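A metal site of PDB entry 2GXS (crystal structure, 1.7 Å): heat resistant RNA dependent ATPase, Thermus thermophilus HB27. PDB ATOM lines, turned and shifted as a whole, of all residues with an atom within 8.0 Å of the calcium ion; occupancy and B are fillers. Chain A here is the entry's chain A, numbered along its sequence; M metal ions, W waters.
O of Gly 160 binds the calcium ion (2.3 Å). Water W3 binds the calcium ion, 2.4 Å away. The calcium ion is bound by OE1 of Glu 163 (2.5 Å). Water W1 binds the calcium ion (2.5 Å). The calcium ion is bound by the side-chain carboxylate (OE1) of Glu 164 (2.5 Å). Water W2 binds the calcium ion (2.5 Å). The calcium ion is bound by the side-chain carboxylate (OE2) of Glu 164 (2.6 Å).
Of the 12 residues printed, 3 come within 4 Å of the calcium ion.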
ATOM      1  N   PRO A 128     -10.337 -27.605   3.628  1.00  0.00           N
ATOM      2  CA  PRO A 128      -9.329 -26.564   3.875  1.00  0.00           C
ATOM      3  C   PRO A 128      -8.219 -26.937   4.899  1.00  0.00           C
ATOM      4  O   PRO A 128      -7.072 -26.510   4.755  1.00  0.00           O
ATOM      5  CB  PRO A 128     -10.145 -25.362   4.342  1.00  0.00           C
ATOM      6  CG  PRO A 128     -11.509 -25.642   3.879  1.00  0.00           C
ATOM      7  CD  PRO A 128     -11.685 -27.135   3.981  1.00  0.00           C
ATOM      8  N   GLY A 129      -8.570 -27.738   5.872  1.00  0.00           N
ATOM      9  CA  GLY A 129      -7.606 -28.132   6.908  1.00  0.00           C
ATOM     10  C   GLY A 129      -6.494 -28.980   6.333  1.00  0.00           C
ATOM     11  O   GLY A 129      -5.307 -28.697   6.491  1.00  0.00           O
ATOM     12  N   LEU A 132      -4.320 -27.168   3.893  1.00  0.00           N
ATOM     13  CA  LEU A 132      -3.337 -26.232   4.449  1.00  0.00           C
ATOM     14  C   LEU A 132      -2.131 -27.025   4.946  1.00  0.00           C
ATOM     15  O   LEU A 132      -1.001 -26.559   4.825  1.00  0.00           O
ATOM     16  CB  LEU A 132      -3.923 -25.343   5.556  1.00  0.00           C
ATOM     17  CG  LEU A 132      -3.004 -24.264   6.151  1.00  0.00           C
ATOM     18  CD1 LEU A 132      -2.540 -23.289   5.099  1.00  0.00           C
ATOM     19  CD2 LEU A 132      -3.725 -23.486   7.309  1.00  0.00           C
ATOM     20  N   MET A 156     -18.103 -23.546   5.196  1.00  0.00           N
ATOM     21  CA  MET A 156     -16.673 -23.503   5.552  1.00  0.00           C
ATOM     22  C   MET A 156     -16.492 -22.570   6.786  1.00  0.00           C
ATOM     23  O   MET A 156     -15.737 -22.849   7.732  1.00  0.00           O
ATOM     24  CB  MET A 156     -15.826 -23.069   4.344  1.00  0.00           C
ATOM     25  CG  MET A 156     -15.747 -24.189   3.323  1.00  0.00           C
ATOM     26  SD  MET A 156     -14.453 -24.109   2.090  1.00  0.00           S
ATOM     27  CE  MET A 156     -14.970 -22.674   1.211  1.00  0.00           C
ATOM     28  N   LEU A 157     -17.242 -21.465   6.768  1.00  0.00           N
ATOM     29  CA  LEU A 157     -17.223 -20.523   7.868  1.00  0.00           C
ATOM     30  C   LEU A 157     -17.737 -21.209   9.115  1.00  0.00           C
ATOM     31  O   LEU A 157     -17.121 -21.160  10.184  1.00  0.00           O
ATOM     32  CB  LEU A 157     -18.131 -19.352   7.539  1.00  0.00           C
ATOM     33  CG  LEU A 157     -18.311 -18.330   8.673  1.00  0.00           C
ATOM     34  CD1 LEU A 157     -16.984 -17.666   8.979  1.00  0.00           C
ATOM     35  CD2 LEU A 157     -19.405 -17.335   8.229  1.00  0.00           C
ATOM     36  N   MET A 159     -17.833 -24.151  10.076  1.00  0.00           N
ATOM     37  CA  MET A 159     -16.942 -25.209  10.577  1.00  0.00           C
ATOM     38  C   MET A 159     -15.610 -24.737  11.096  1.00  0.00           C
ATOM     39  O   MET A 159     -14.799 -25.532  11.602  1.00  0.00           O
ATOM     40  CB  MET A 159     -16.618 -26.154   9.446  1.00  0.00           C
ATOM     41  CG  MET A 159     -17.772 -26.897   9.027  1.00  0.00           C
ATOM     42  SD  MET A 159     -17.337 -27.673   7.518  1.00  0.00           S
ATOM     43  CE  MET A 159     -17.922 -29.335   7.845  1.00  0.00           C
ATOM     44  N   GLY A 160     -15.348 -23.452  10.957  1.00  0.00           N
ATOM     45  CA  GLY A 160     -14.147 -22.862  11.487  1.00  0.00           C
ATOM     46  C   GLY A 160     -12.995 -22.801  10.522  1.00  0.00           C
ATOM     47  O   GLY A 160     -11.856 -22.662  10.943  1.00  0.00           O
ATOM     48  N   PHE A 161     -13.266 -22.867   9.210  1.00  0.00           N
ATOM     49  CA  PHE A 161     -12.184 -22.877   8.201  1.00  0.00           C
ATOM     50  C   PHE A 161     -11.764 -21.494   7.650  1.00  0.00           C
ATOM     51  O   PHE A 161     -11.035 -21.375   6.657  1.00  0.00           O
ATOM     52  CB  PHE A 161     -12.535 -23.790   7.037  1.00  0.00           C
ATOM     53  CG  PHE A 161     -12.634 -25.239   7.392  1.00  0.00           C
ATOM     54  CD1 PHE A 161     -11.608 -25.867   8.107  1.00  0.00           C
ATOM     55  CD2 PHE A 161     -13.703 -25.980   6.954  1.00  0.00           C
ATOM     56  CE1 PHE A 161     -11.695 -27.208   8.394  1.00  0.00           C
ATOM     57  CE2 PHE A 161     -13.818 -27.309   7.260  1.00  0.00           C
ATOM     58  CZ  PHE A 161     -12.814 -27.924   7.973  1.00  0.00           C
ATOM     59  N   GLU A 162     -12.208 -20.419   8.314  1.00  0.00           N
ATOM     60  CA  GLU A 162     -11.965 -19.091   7.792  1.00  0.00           C
ATOM     61  C   GLU A 162     -10.453 -18.872   7.576  1.00  0.00           C
ATOM     62  O   GLU A 162     -10.035 -18.393   6.527  1.00  0.00           O
ATOM     63  CB  GLU A 162     -12.668 -18.020   8.662  1.00  0.00           C
ATOM     64  CG  GLU A 162     -12.490 -18.167  10.200  1.00  0.00           C
ATOM     65  CD  GLU A 162     -13.365 -17.218  10.985  1.00  0.00           C
ATOM     66  OE1 GLU A 162     -13.030 -16.029  11.221  1.00  0.00           O
ATOM     67  OE2 GLU A 162     -14.393 -17.658  11.377  1.00  0.00           O
ATOM     68  N   GLU A 163      -9.644 -19.267   8.550  1.00  0.00           N
ATOM     69  CA  GLU A 163      -8.229 -18.983   8.502  1.00  0.00           C
ATOM     70  C   GLU A 163      -7.544 -19.781   7.416  1.00  0.00           C
ATOM     71  O   GLU A 163      -6.688 -19.281   6.699  1.00  0.00           O
ATOM     72  CB  GLU A 163      -7.583 -19.261   9.863  1.00  0.00           C
ATOM     73  CG  GLU A 163      -8.282 -18.515  11.032  1.00  0.00           C
ATOM     74  CD  GLU A 163      -9.462 -19.245  11.700  1.00  0.00           C
ATOM     75  OE1 GLU A 163      -9.890 -20.307  11.219  1.00  0.00           O
ATOM     76  OE2 GLU A 163      -9.944 -18.724  12.751  1.00  0.00           O
ATOM     77  N   GLU A 164      -7.953 -21.043   7.299  1.00  0.00           N
ATOM     78  CA  GLU A 164      -7.324 -21.970   6.347  1.00  0.00           C
ATOM     79  C   GLU A 164      -7.635 -21.507   4.905  1.00  0.00           C
ATOM     80  O   GLU A 164      -6.778 -21.461   4.010  1.00  0.00           O
ATOM     81  CB  GLU A 164      -7.858 -23.370   6.562  1.00  0.00           C
ATOM     82  CG  GLU A 164      -7.420 -24.065   7.898  1.00  0.00           C
ATOM     83  CD  GLU A 164      -8.160 -23.601   9.168  1.00  0.00           C
ATOM     84  OE1 GLU A 164      -9.208 -22.935   9.117  1.00  0.00           O
ATOM     85  OE2 GLU A 164      -7.658 -23.898  10.278  1.00  0.00           O
ATOM     86  N   VAL A 165      -8.901 -21.170   4.691  1.00  0.00           N
ATOM     87  CA  VAL A 165      -9.313 -20.668   3.391  1.00  0.00           C
ATOM     88  C   VAL A 165      -8.592 -19.397   2.976  1.00  0.00           C
ATOM     89  O   VAL A 165      -8.137 -19.276   1.839  1.00  0.00           O
ATOM     90  CB  VAL A 165     -10.862 -20.439   3.343  1.00  0.00           C
ATOM     91  CG1 VAL A 165     -11.230 -19.621   2.110  1.00  0.00           C
ATOM     92  CG2 VAL A 165     -11.605 -21.778   3.380  1.00  0.00           C
HETATM   93 CA    CA M   1      -9.629 -22.720  11.578  1.00  0.00          CA
HETATM   94  O   HOH W   1     -10.826 -22.791  13.774  1.00  0.00           O
HETATM   95  O   HOH W   2      -8.145 -23.162  13.604  1.00  0.00           O
HETATM   96  O   HOH W   3     -10.149 -25.060  11.818  1.00  0.00           O
